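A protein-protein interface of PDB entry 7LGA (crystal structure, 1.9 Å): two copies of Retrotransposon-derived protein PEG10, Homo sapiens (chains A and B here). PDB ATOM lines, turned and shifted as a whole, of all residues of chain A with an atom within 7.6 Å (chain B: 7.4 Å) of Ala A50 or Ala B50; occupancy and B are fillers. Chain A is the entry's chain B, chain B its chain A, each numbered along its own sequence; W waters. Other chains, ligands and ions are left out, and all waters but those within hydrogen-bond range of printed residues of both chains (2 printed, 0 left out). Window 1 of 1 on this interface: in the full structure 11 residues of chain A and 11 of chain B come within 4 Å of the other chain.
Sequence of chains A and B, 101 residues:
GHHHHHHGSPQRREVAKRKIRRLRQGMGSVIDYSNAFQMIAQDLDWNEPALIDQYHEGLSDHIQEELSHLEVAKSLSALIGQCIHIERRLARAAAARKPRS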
ATOM      1  N   ARG A  21     -22.899  11.276  14.124  1.00  0.00           N
ATOM      2  CA  ARG A  21     -23.474  10.784  15.366  1.00  0.00           C
ATOM      3  C   ARG A  21     -24.775  11.479  15.671  1.00  0.00           C
ATOM      4  O   ARG A  21     -25.676  10.864  16.254  1.00  0.00           O
ATOM      5  CB  ARG A  21     -22.506  10.977  16.525  1.00  0.00           C
ATOM      6  CG  ARG A  21     -21.782   9.730  16.853  1.00  0.00           C
ATOM      7  CD  ARG A  21     -20.905   9.921  18.081  1.00  0.00           C
ATOM      8  NE  ARG A  21     -19.658   9.222  17.849  1.00  0.00           N
ATOM      9  CZ  ARG A  21     -19.524   7.908  17.939  1.00  0.00           C
ATOM     10  NH1 ARG A  21     -20.557   7.153  18.306  1.00  0.00           N
ATOM     11  NH2 ARG A  21     -18.352   7.360  17.674  1.00  0.00           N
ATOM     12  N   PHE A  37     -26.412  10.912   5.035  1.00  0.00           N
ATOM     13  CA  PHE A  37     -25.470  10.004   5.678  1.00  0.00           C
ATOM     14  C   PHE A  37     -24.263   9.750   4.788  1.00  0.00           C
ATOM     15  O   PHE A  37     -23.120   9.806   5.247  1.00  0.00           O
ATOM     16  CB  PHE A  37     -26.154   8.672   6.033  1.00  0.00           C
ATOM     17  CG  PHE A  37     -25.285   7.750   6.857  1.00  0.00           C
ATOM     18  CD1 PHE A  37     -25.401   7.704   8.242  1.00  0.00           C
ATOM     19  CD2 PHE A  37     -24.340   6.949   6.250  1.00  0.00           C
ATOM     20  CE1 PHE A  37     -24.588   6.869   8.993  1.00  0.00           C
ATOM     21  CE2 PHE A  37     -23.518   6.123   7.000  1.00  0.00           C
ATOM     22  CZ  PHE A  37     -23.647   6.082   8.371  1.00  0.00           C
ATOM     23  N   ASP A  45     -13.086   8.029   8.164  1.00  0.00           N
ATOM     24  CA  ASP A  45     -12.223   6.879   7.953  1.00  0.00           C
ATOM     25  C   ASP A  45     -12.726   5.645   8.699  1.00  0.00           C
ATOM     26  O   ASP A  45     -11.963   4.698   8.911  1.00  0.00           O
ATOM     27  CB  ASP A  45     -10.788   7.206   8.370  1.00  0.00           C
ATOM     28  CG  ASP A  45     -10.691   7.748   9.783  1.00  0.00           C
ATOM     29  OD1 ASP A  45     -11.734   8.090  10.374  1.00  0.00           O
ATOM     30  OD2 ASP A  45      -9.560   7.838  10.303  1.00  0.00           O
ATOM     31  N   TRP A  46     -13.990   5.644   9.107  1.00  0.00           N
ATOM     32  CA  TRP A  46     -14.588   4.455   9.700  1.00  0.00           C
ATOM     33  C   TRP A  46     -14.762   3.376   8.639  1.00  0.00           C
ATOM     34  O   TRP A  46     -15.019   3.671   7.472  1.00  0.00           O
ATOM     35  CB  TRP A  46     -15.953   4.774  10.289  1.00  0.00           C
ATOM     36  CG  TRP A  46     -15.987   5.782  11.378  1.00  0.00           C
ATOM     37  CD1 TRP A  46     -14.935   6.447  11.938  1.00  0.00           C
ATOM     38  CD2 TRP A  46     -17.157   6.234  12.055  1.00  0.00           C
ATOM     39  NE1 TRP A  46     -15.387   7.291  12.919  1.00  0.00           N
ATOM     40  CE2 TRP A  46     -16.749   7.171  13.014  1.00  0.00           C
ATOM     41  CE3 TRP A  46     -18.514   5.922  11.950  1.00  0.00           C
ATOM     42  CZ2 TRP A  46     -17.650   7.812  13.856  1.00  0.00           C
ATOM     43  CZ3 TRP A  46     -19.404   6.554  12.785  1.00  0.00           C
ATOM     44  CH2 TRP A  46     -18.972   7.492  13.722  1.00  0.00           C
ATOM     45  N   ASN A  47     -14.622   2.114   9.040  1.00  0.00           N
ATOM     46  CA  ASN A  47     -14.830   1.036   8.086  1.00  0.00           C
ATOM     47  C   ASN A  47     -16.328   0.761   7.930  1.00  0.00           C
ATOM     48  O   ASN A  47     -17.177   1.354   8.607  1.00  0.00           O
ATOM     49  CB  ASN A  47     -14.047  -0.213   8.496  1.00  0.00           C
ATOM     50  CG  ASN A  47     -14.546  -0.842   9.778  1.00  0.00           C
ATOM     51  OD1 ASN A  47     -15.264  -0.226  10.567  1.00  0.00           O
ATOM     52  ND2 ASN A  47     -14.130  -2.077  10.009  1.00  0.00           N
ATOM     53  N   GLU A  48     -16.662  -0.149   7.016  1.00  0.00           N
ATOM     54  CA  GLU A  48     -18.052  -0.339   6.626  1.00  0.00           C
ATOM     55  C   GLU A  48     -18.904  -0.917   7.757  1.00  0.00           C
ATOM     56  O   GLU A  48     -20.073  -0.538   7.896  1.00  0.00           O
ATOM     57  CB  GLU A  48     -18.141  -1.233   5.381  1.00  0.00           C
ATOM     58  CG  GLU A  48     -19.549  -1.278   4.797  1.00  0.00           C
ATOM     59  CD  GLU A  48     -19.591  -1.801   3.373  1.00  0.00           C
ATOM     60  OE1 GLU A  48     -18.542  -2.260   2.862  1.00  0.00           O
ATOM     61  OE2 GLU A  48     -20.664  -1.701   2.747  1.00  0.00           O
ATOM     62  N   PRO A  49     -18.386  -1.841   8.566  1.00  0.00           N
ATOM     63  CA  PRO A  49     -19.177  -2.305   9.725  1.00  0.00           C
ATOM     64  C   PRO A  49     -19.593  -1.182  10.671  1.00  0.00           C
ATOM     65  O   PRO A  49     -20.760  -1.122  11.105  1.00  0.00           O
ATOM     66  CB  PRO A  49     -18.231  -3.308  10.400  1.00  0.00           C
ATOM     67  CG  PRO A  49     -17.392  -3.850   9.270  1.00  0.00           C
ATOM     68  CD  PRO A  49     -17.214  -2.703   8.303  1.00  0.00           C
ATOM     69  N   ALA A  50     -18.661  -0.280  10.994  1.00  0.00           N
ATOM     70  CA  ALA A  50     -18.980   0.853  11.853  1.00  0.00           C
ATOM     71  C   ALA A  50     -19.998   1.773  11.195  1.00  0.00           C
ATOM     72  O   ALA A  50     -20.922   2.254  11.857  1.00  0.00           O
ATOM     73  CB  ALA A  50     -17.707   1.622  12.197  1.00  0.00           C
ATOM     74  N   LEU A  51     -19.860   2.004   9.886  1.00  0.00           N
ATOM     75  CA  LEU A  51     -20.810   2.862   9.189  1.00  0.00           C
ATOM     76  C   LEU A  51     -22.196   2.235   9.150  1.00  0.00           C
ATOM     77  O   LEU A  51     -23.193   2.939   9.308  1.00  0.00           O
ATOM     78  CB  LEU A  51     -20.324   3.152   7.773  1.00  0.00           C
ATOM     79  CG  LEU A  51     -19.091   4.050   7.616  1.00  0.00           C
ATOM     80  CD1 LEU A  51     -18.639   4.031   6.157  1.00  0.00           C
ATOM     81  CD2 LEU A  51     -19.376   5.469   8.081  1.00  0.00           C
ATOM     82  N   ILE A  52     -22.272   0.920   8.929  1.00  0.00           N
ATOM     83  CA  ILE A  52     -23.552   0.213   8.928  1.00  0.00           C
ATOM     84  C   ILE A  52     -24.238   0.370  10.274  1.00  0.00           C
ATOM     85  O   ILE A  52     -25.434   0.674  10.352  1.00  0.00           O
ATOM     86  CB  ILE A  52     -23.340  -1.275   8.596  1.00  0.00           C
ATOM     87  CG1 ILE A  52     -23.045  -1.466   7.109  1.00  0.00           C
ATOM     88  CG2 ILE A  52     -24.543  -2.102   9.041  1.00  0.00           C
ATOM     89  CD1 ILE A  52     -22.564  -2.878   6.774  1.00  0.00           C
ATOM     90  N   ASP A  53     -23.488   0.153  11.356  1.00  0.00           N
ATOM     91  CA  ASP A  53     -24.065   0.264  12.692  1.00  0.00           C
ATOM     92  C   ASP A  53     -24.535   1.687  12.994  1.00  0.00           C
ATOM     93  O   ASP A  53     -25.619   1.878  13.562  1.00  0.00           O
ATOM     94  CB  ASP A  53     -23.040  -0.229  13.717  1.00  0.00           C
ATOM     95  CG  ASP A  53     -22.796  -1.733  13.610  1.00  0.00           C
ATOM     96  OD1 ASP A  53     -23.608  -2.434  12.970  1.00  0.00           O
ATOM     97  OD2 ASP A  53     -21.789  -2.216  14.162  1.00  0.00           O
ATOM     98  N   GLN A  54     -23.748   2.699  12.616  1.00  0.00           N
ATOM     99  CA  GLN A  54     -24.196   4.077  12.801  1.00  0.00           C
ATOM    100  C   GLN A  54     -25.441   4.371  11.971  1.00  0.00           C
ATOM    101  O   GLN A  54     -26.381   5.025  12.445  1.00  0.00           O
ATOM    102  CB  GLN A  54     -23.081   5.055  12.427  1.00  0.00           C
ATOM    103  CG  GLN A  54     -23.472   6.497  12.685  1.00  0.00           C
ATOM    104  CD  GLN A  54     -23.650   6.770  14.164  1.00  0.00           C
ATOM    105  OE1 GLN A  54     -22.716   6.609  14.950  1.00  0.00           O
ATOM    106  NE2 GLN A  54     -24.854   7.161  14.556  1.00  0.00           N
ATOM    107  N   TYR A  55     -25.468   3.900  10.723  1.00  0.00           N
ATOM    108  CA  TYR A  55     -26.632   4.118   9.870  1.00  0.00           C
ATOM    109  C   TYR A  55     -27.879   3.513  10.494  1.00  0.00           C
ATOM    110  O   TYR A  55     -28.947   4.138  10.537  1.00  0.00           O
ATOM    111  CB  TYR A  55     -26.375   3.512   8.487  1.00  0.00           C
ATOM    112  CG  TYR A  55     -27.547   3.634   7.552  1.00  0.00           C
ATOM    113  CD1 TYR A  55     -27.667   4.715   6.701  1.00  0.00           C
ATOM    114  CD2 TYR A  55     -28.546   2.666   7.529  1.00  0.00           C
ATOM    115  CE1 TYR A  55     -28.765   4.830   5.841  1.00  0.00           C
ATOM    116  CE2 TYR A  55     -29.619   2.764   6.676  1.00  0.00           C
ATOM    117  CZ  TYR A  55     -29.727   3.844   5.837  1.00  0.00           C
ATOM    118  OH  TYR A  55     -30.813   3.936   5.002  1.00  0.00           O
ATOM    119  N   HIS A  56     -27.759   2.283  10.985  1.00  0.00           N
ATOM    120  CA  HIS A  56     -28.900   1.650  11.633  1.00  0.00           C
ATOM    121  C   HIS A  56     -29.333   2.441  12.867  1.00  0.00           C
ATOM    122  O   HIS A  56     -30.534   2.608  13.115  1.00  0.00           O
ATOM    123  CB  HIS A  56     -28.559   0.201  11.997  1.00  0.00           C
ATOM    124  CG  HIS A  56     -29.705  -0.545  12.606  1.00  0.00           C
ATOM    125  ND1 HIS A  56     -30.041  -0.438  13.939  1.00  0.00           N
ATOM    126  CD2 HIS A  56     -30.605  -1.397  12.060  1.00  0.00           C
ATOM    127  CE1 HIS A  56     -31.101  -1.188  14.185  1.00  0.00           C
ATOM    128  NE2 HIS A  56     -31.462  -1.781  13.062  1.00  0.00           N
ATOM    129  N   LEU A  76     -23.343  -1.491   3.355  1.00  0.00           N
ATOM    130  CA  LEU A  76     -24.078  -0.250   3.575  1.00  0.00           C
ATOM    131  C   LEU A  76     -24.981   0.086   2.396  1.00  0.00           C
ATOM    132  O   LEU A  76     -26.127   0.510   2.584  1.00  0.00           O
ATOM    133  CB  LEU A  76     -23.098   0.893   3.843  1.00  0.00           C
ATOM    134  CG  LEU A  76     -23.702   2.273   4.077  1.00  0.00           C
ATOM    135  CD1 LEU A  76     -24.639   2.248   5.274  1.00  0.00           C
ATOM    136  CD2 LEU A  76     -22.580   3.278   4.259  1.00  0.00           C
ATOM    137  N   ARG B  13     -21.658 -10.020  17.975  1.00  0.00           N
ATOM    138  CA  ARG B  13     -21.416  -8.740  17.312  1.00  0.00           C
ATOM    139  C   ARG B  13     -22.582  -7.778  17.519  1.00  0.00           C
ATOM    140  O   ARG B  13     -22.374  -6.586  17.781  1.00  0.00           O
ATOM    141  CB  ARG B  13     -21.164  -8.979  15.820  1.00  0.00           C
ATOM    142  CG  ARG B  13     -20.230  -7.983  15.137  1.00  0.00           C
ATOM    143  CD  ARG B  13     -20.633  -7.778  13.664  1.00  0.00           C
ATOM    144  NE  ARG B  13     -21.929  -7.105  13.586  1.00  0.00           N
ATOM    145  CZ  ARG B  13     -22.092  -5.784  13.500  1.00  0.00           C
ATOM    146  NH1 ARG B  13     -23.317  -5.265  13.466  1.00  0.00           N
ATOM    147  NH2 ARG B  13     -21.034  -4.979  13.443  1.00  0.00           N
ATOM    148  N   ILE B  20     -21.393  -1.184  23.270  1.00  0.00           N
ATOM    149  CA  ILE B  20     -20.297  -0.226  23.149  1.00  0.00           C
ATOM    150  C   ILE B  20     -20.849   1.185  23.018  1.00  0.00           C
ATOM    151  O   ILE B  20     -20.275   2.152  23.539  1.00  0.00           O
ATOM    152  CB  ILE B  20     -19.400  -0.595  21.957  1.00  0.00           C
ATOM    153  CG1 ILE B  20     -18.021   0.053  22.096  1.00  0.00           C
ATOM    154  CG2 ILE B  20     -20.007  -0.119  20.671  1.00  0.00           C
ATOM    155  CD1 ILE B  20     -16.991  -0.799  22.762  1.00  0.00           C
ATOM    156  N   ARG B  21     -21.984   1.322  22.333  1.00  0.00           N
ATOM    157  CA  ARG B  21     -22.565   2.635  22.121  1.00  0.00           C
ATOM    158  C   ARG B  21     -23.164   3.184  23.405  1.00  0.00           C
ATOM    159  O   ARG B  21     -23.220   4.404  23.580  1.00  0.00           O
ATOM    160  CB  ARG B  21     -23.620   2.573  21.014  1.00  0.00           C
ATOM    161  CG  ARG B  21     -23.863   3.900  20.350  1.00  0.00           C
ATOM    162  CD  ARG B  21     -24.793   3.759  19.170  1.00  0.00           C
ATOM    163  NE  ARG B  21     -24.141   3.162  18.010  1.00  0.00           N
ATOM    164  CZ  ARG B  21     -23.428   3.850  17.124  1.00  0.00           C
ATOM    165  NH1 ARG B  21     -23.251   5.153  17.274  1.00  0.00           N
ATOM    166  NH2 ARG B  21     -22.885   3.235  16.086  1.00  0.00           N
ATOM    167  N   PHE B  37     -14.504  -1.183  27.712  1.00  0.00           N
ATOM    168  CA  PHE B  37     -14.576  -0.845  26.296  1.00  0.00           C
ATOM    169  C   PHE B  37     -13.869  -1.901  25.460  1.00  0.00           C
ATOM    170  O   PHE B  37     -14.411  -2.388  24.461  1.00  0.00           O
ATOM    171  CB  PHE B  37     -13.961   0.547  26.076  1.00  0.00           C
ATOM    172  CG  PHE B  37     -14.077   1.058  24.671  1.00  0.00           C
ATOM    173  CD1 PHE B  37     -15.107   1.919  24.330  1.00  0.00           C
ATOM    174  CD2 PHE B  37     -13.154   0.695  23.700  1.00  0.00           C
ATOM    175  CE1 PHE B  37     -15.225   2.399  23.063  1.00  0.00           C
ATOM    176  CE2 PHE B  37     -13.271   1.167  22.426  1.00  0.00           C
ATOM    177  CZ  PHE B  37     -14.311   2.020  22.099  1.00  0.00           C
ATOM    178  N   ASP B  45     -16.239  -5.694  14.892  1.00  0.00           N
ATOM    179  CA  ASP B  45     -15.424  -5.636  13.686  1.00  0.00           C
ATOM    180  C   ASP B  45     -15.194  -4.202  13.224  1.00  0.00           C
ATOM    181  O   ASP B  45     -14.854  -3.969  12.059  1.00  0.00           O
ATOM    182  CB  ASP B  45     -16.075  -6.464  12.576  1.00  0.00           C
ATOM    183  CG  ASP B  45     -17.546  -6.138  12.389  1.00  0.00           C
ATOM    184  OD1 ASP B  45     -18.105  -5.364  13.211  1.00  0.00           O
ATOM    185  OD2 ASP B  45     -18.145  -6.651  11.417  1.00  0.00           O
ATOM    186  N   TRP B  46     -15.385  -3.235  14.113  1.00  0.00           N
ATOM    187  CA  TRP B  46     -15.065  -1.855  13.796  1.00  0.00           C
ATOM    188  C   TRP B  46     -13.556  -1.668  13.714  1.00  0.00           C
ATOM    189  O   TRP B  46     -12.794  -2.311  14.435  1.00  0.00           O
ATOM    190  CB  TRP B  46     -15.604  -0.914  14.862  1.00  0.00           C
ATOM    191  CG  TRP B  46     -17.083  -0.853  15.028  1.00  0.00           C
ATOM    192  CD1 TRP B  46     -18.028  -1.615  14.412  1.00  0.00           C
ATOM    193  CD2 TRP B  46     -17.780   0.012  15.920  1.00  0.00           C
ATOM    194  NE1 TRP B  46     -19.285  -1.265  14.860  1.00  0.00           N
ATOM    195  CE2 TRP B  46     -19.156  -0.266  15.788  1.00  0.00           C
ATOM    196  CE3 TRP B  46     -17.371   1.001  16.818  1.00  0.00           C
ATOM    197  CZ2 TRP B  46     -20.128   0.418  16.516  1.00  0.00           C
ATOM    198  CZ3 TRP B  46     -18.339   1.686  17.537  1.00  0.00           C
ATOM    199  CH2 TRP B  46     -19.699   1.388  17.387  1.00  0.00           C
ATOM    200  N   ASN B  47     -13.122  -0.765  12.840  1.00  0.00           N
ATOM    201  CA  ASN B  47     -11.701  -0.490  12.728  1.00  0.00           C
ATOM    202  C   ASN B  47     -11.272   0.508  13.801  1.00  0.00           C
ATOM    203  O   ASN B  47     -12.083   1.047  14.559  1.00  0.00           O
ATOM    204  CB  ASN B  47     -11.352   0.005  11.318  1.00  0.00           C
ATOM    205  CG  ASN B  47     -11.947   1.367  10.985  1.00  0.00           C
ATOM    206  OD1 ASN B  47     -12.856   1.858  11.649  1.00  0.00           O
ATOM    207  ND2 ASN B  47     -11.436   1.978   9.918  1.00  0.00           N
ATOM    208  N   GLU B  48      -9.978   0.741  13.875  1.00  0.00           N
ATOM    209  CA  GLU B  48      -9.454   1.499  15.001  1.00  0.00           C
ATOM    210  C   GLU B  48      -9.926   2.949  15.004  1.00  0.00           C
ATOM    211  O   GLU B  48     -10.210   3.488  16.075  1.00  0.00           O
ATOM    212  CB  GLU B  48      -7.923   1.442  15.036  1.00  0.00           C
ATOM    213  CG  GLU B  48      -7.377   1.868  16.397  1.00  0.00           C
ATOM    214  CD  GLU B  48      -6.005   1.325  16.679  1.00  0.00           C
ATOM    215  OE1 GLU B  48      -5.319   0.916  15.724  1.00  0.00           O
ATOM    216  OE2 GLU B  48      -5.601   1.342  17.853  1.00  0.00           O
ATOM    217  N   PRO B  49     -10.051   3.619  13.857  1.00  0.00           N
ATOM    218  CA  PRO B  49     -10.645   4.969  13.888  1.00  0.00           C
ATOM    219  C   PRO B  49     -12.042   5.030  14.508  1.00  0.00           C
ATOM    220  O   PRO B  49     -12.327   5.924  15.323  1.00  0.00           O
ATOM    221  CB  PRO B  49     -10.652   5.365  12.403  1.00  0.00           C
ATOM    222  CG  PRO B  49      -9.475   4.646  11.831  1.00  0.00           C
ATOM    223  CD  PRO B  49      -9.396   3.325  12.568  1.00  0.00           C
ATOM    224  N   ALA B  50     -12.931   4.103  14.141  1.00  0.00           N
ATOM    225  CA  ALA B  50     -14.273   4.097  14.719  1.00  0.00           C
ATOM    226  C   ALA B  50     -14.234   3.819  16.218  1.00  0.00           C
ATOM    227  O   ALA B  50     -14.990   4.419  16.989  1.00  0.00           O
ATOM    228  CB  ALA B  50     -15.134   3.059  14.008  1.00  0.00           C
ATOM    229  N   LEU B  51     -13.350   2.926  16.652  1.00  0.00           N
ATOM    230  CA  LEU B  51     -13.213   2.651  18.075  1.00  0.00           C
ATOM    231  C   LEU B  51     -12.652   3.854  18.824  1.00  0.00           C
ATOM    232  O   LEU B  51     -13.086   4.159  19.939  1.00  0.00           O
ATOM    233  CB  LEU B  51     -12.312   1.437  18.266  1.00  0.00           C
ATOM    234  CG  LEU B  51     -12.840   0.064  17.866  1.00  0.00           C
ATOM    235  CD1 LEU B  51     -11.700  -0.943  18.006  1.00  0.00           C
ATOM    236  CD2 LEU B  51     -14.051  -0.369  18.667  1.00  0.00           C
ATOM    237  N   ILE B  52     -11.668   4.541  18.245  1.00  0.00           N
ATOM    238  CA  ILE B  52     -11.147   5.750  18.877  1.00  0.00           C
ATOM    239  C   ILE B  52     -12.272   6.755  19.083  1.00  0.00           C
ATOM    240  O   ILE B  52     -12.423   7.345  20.164  1.00  0.00           O
ATOM    241  CB  ILE B  52     -10.012   6.362  18.036  1.00  0.00           C
ATOM    242  CG1 ILE B  52      -8.733   5.535  18.163  1.00  0.00           C
ATOM    243  CG2 ILE B  52      -9.791   7.818  18.461  1.00  0.00           C
ATOM    244  CD1 ILE B  52      -7.693   5.882  17.107  1.00  0.00           C
ATOM    245  N   ASP B  53     -13.072   6.977  18.042  1.00  0.00           N
ATOM    246  CA  ASP B  53     -14.115   7.992  18.145  1.00  0.00           C
ATOM    247  C   ASP B  53     -15.202   7.583  19.138  1.00  0.00           C
ATOM    248  O   ASP B  53     -15.708   8.422  19.891  1.00  0.00           O
ATOM    249  CB  ASP B  53     -14.682   8.277  16.761  1.00  0.00           C
ATOM    250  CG  ASP B  53     -13.672   8.988  15.860  1.00  0.00           C
ATOM    251  OD1 ASP B  53     -12.702   9.559  16.404  1.00  0.00           O
ATOM    252  OD2 ASP B  53     -13.839   8.976  14.622  1.00  0.00           O
ATOM    253  N   GLN B  54     -15.549   6.296  19.194  1.00  0.00           N
ATOM    254  CA  GLN B  54     -16.534   5.868  20.188  1.00  0.00           C
ATOM    255  C   GLN B  54     -15.976   6.002  21.606  1.00  0.00           C
ATOM    256  O   GLN B  54     -16.658   6.493  22.522  1.00  0.00           O
ATOM    257  CB  GLN B  54     -16.967   4.426  19.911  1.00  0.00           C
ATOM    258  CG  GLN B  54     -18.073   3.957  20.847  1.00  0.00           C
ATOM    259  CD  GLN B  54     -19.341   4.765  20.658  1.00  0.00           C
ATOM    260  OE1 GLN B  54     -19.901   4.815  19.559  1.00  0.00           O
ATOM    261  NE2 GLN B  54     -19.785   5.418  21.714  1.00  0.00           N
ATOM    262  N   TYR B  55     -14.726   5.579  21.801  1.00  0.00           N
ATOM    263  CA  TYR B  55     -14.095   5.691  23.110  1.00  0.00           C
ATOM    264  C   TYR B  55     -14.128   7.129  23.587  1.00  0.00           C
ATOM    265  O   TYR B  55     -14.515   7.410  24.727  1.00  0.00           O
ATOM    266  CB  TYR B  55     -12.653   5.182  23.039  1.00  0.00           C
ATOM    267  CG  TYR B  55     -11.898   5.279  24.336  1.00  0.00           C
ATOM    268  CD1 TYR B  55     -11.816   4.194  25.184  1.00  0.00           C
ATOM    269  CD2 TYR B  55     -11.275   6.460  24.716  1.00  0.00           C
ATOM    270  CE1 TYR B  55     -11.136   4.274  26.375  1.00  0.00           C
ATOM    271  CE2 TYR B  55     -10.584   6.548  25.898  1.00  0.00           C
ATOM    272  CZ  TYR B  55     -10.520   5.451  26.726  1.00  0.00           C
ATOM    273  OH  TYR B  55      -9.838   5.535  27.907  1.00  0.00           O
ATOM    274  N   HIS B  56     -13.750   8.062  22.704  1.00  0.00           N
ATOM    275  CA  HIS B  56     -13.785   9.477  23.051  1.00  0.00           C
ATOM    276  C   HIS B  56     -15.198   9.915  23.405  1.00  0.00           C
ATOM    277  O   HIS B  56     -15.406  10.645  24.383  1.00  0.00           O
ATOM    278  CB  HIS B  56     -13.232  10.314  21.890  1.00  0.00           C
ATOM    279  CG  HIS B  56     -13.099  11.772  22.208  1.00  0.00           C
ATOM    280  ND1 HIS B  56     -14.156  12.651  22.114  1.00  0.00           N
ATOM    281  CD2 HIS B  56     -12.044  12.498  22.651  1.00  0.00           C
ATOM    282  CE1 HIS B  56     -13.753  13.859  22.464  1.00  0.00           C
ATOM    283  NE2 HIS B  56     -12.478  13.793  22.800  1.00  0.00           N
HETATM  284  O   HOH W   1     -22.252  -3.963  10.946  1.00  0.00           O
HETATM  285  O   HOH W   2     -23.685   7.495  19.462  1.00  0.00           O
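The guanidinium group (NH1) of Arg B13 is in salt-bridge range of the side-chain carboxylate (OD1) of Asp A53, 2.9 Å away.
The side-chain amide oxygen (OE1) of Gln A54 is in hydrogen-bond range of the guanidinium group (NH1) of Arg B21, at 2.8 Å.
The backbone carbonyl oxygen (O) of Asp B45 is in hydrogen-bond range of the side-chain amide nitrogen (ND2) of Asn A47.
The indole nitrogen of Trp B46 sits at hydrogen-bond distance from the side-chain carboxylate of Asp A53, 2.8 Å away.
ND2 of Asn B47 lies within hydrogen-bond range of O of Asp A45 (2.9 Å).
The side-chain amide oxygen (OD1) of Asn B47 sits at hydrogen-bond distance from the backbone NH (N) of Asn A47, at 3.2 Å.
The indole nitrogen (NE1) of Trp A46 sits at hydrogen-bond distance from the side-chain carboxylate (OD2) of Asp B53 (2.9 Å).
OE1 of Gln B54 is in hydrogen-bond range of NH1 of Arg A21, 2.7 Å away.
The side-chain carboxylate (OD1) of Asp B45 is in salt-bridge range of the guanidinium group (NH2) of Arg B13 (3.0 Å).
OD1 of Asn B47 is in hydrogen-bond range of N of Ala B50.
N of Ala A50 sits at hydrogen-bond distance from OD1 of Asn A47, 3.4 Å away.
Among the printed residues, merely in contact across the chains: Arg A21 with Arg B21 (3.5 Å), Arg A21 with Asp B53 (3.5 Å), Asp A45 with Pro B49 (3.4 Å), Trp A46 with Asn B47 (3.7 Å), Trp A46 with Ala B50 (3.7 Å), Asn A47 with Trp B46 (3.6 Å), Pro A49 with Asp B45 (3.5 Å), Ala A50 with Trp B46 (3.7 Å), Ala A50 with Ala B50 (3.5 Å) and Asp A53 with Arg B21 (3.8 Å).
Of the printed residues of chain B, Ala A50 touches Trp B46 and Ala B50.
Ile A52 touches none of the printed residues of chain B.
Of the printed residues of chain A, Asn B47 touches Asp A45, Trp A46 and Asn A47.
Of the printed residues of chain A, Asp B53 touches Arg A21 and Trp A46.
The nearest printed residue of chain A that does not touch Pro B49 is Trp A46 (4.1 Å).
Of the 15 printed residues of chain A, 8 touch a printed residue of chain B.
Of the 16 printed residues of chain B, 9 touch a printed residue of chain A.
Hydrophobic or aromatic side chains of chain B that line the printed part of chain A: Trp B46, Pro B49 and Ala B50.
Asp A45 touches Pro B49, and with the chains exchanged Pro A49 touches Asp B45.
Trp A46 touches Asn B47, and with the chains exchanged Asn A47 touches Trp B46.
Trp A46 touches Asp B53, and with the chains exchanged Asp A53 touches Trp B46.
Ala A50 touches its own counterpart, Ala B50.
Water W1 lies within hydrogen-bond range of OD1 of Asp A53 (2.9 Å), NH2 of Arg B13 (3.0 Å) and O of Pro A49 (3.2 Å).
Water W2 bridges NH1 of Arg B21 (3.2 Å) and NH1 of Arg A21 (3.4 Å).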
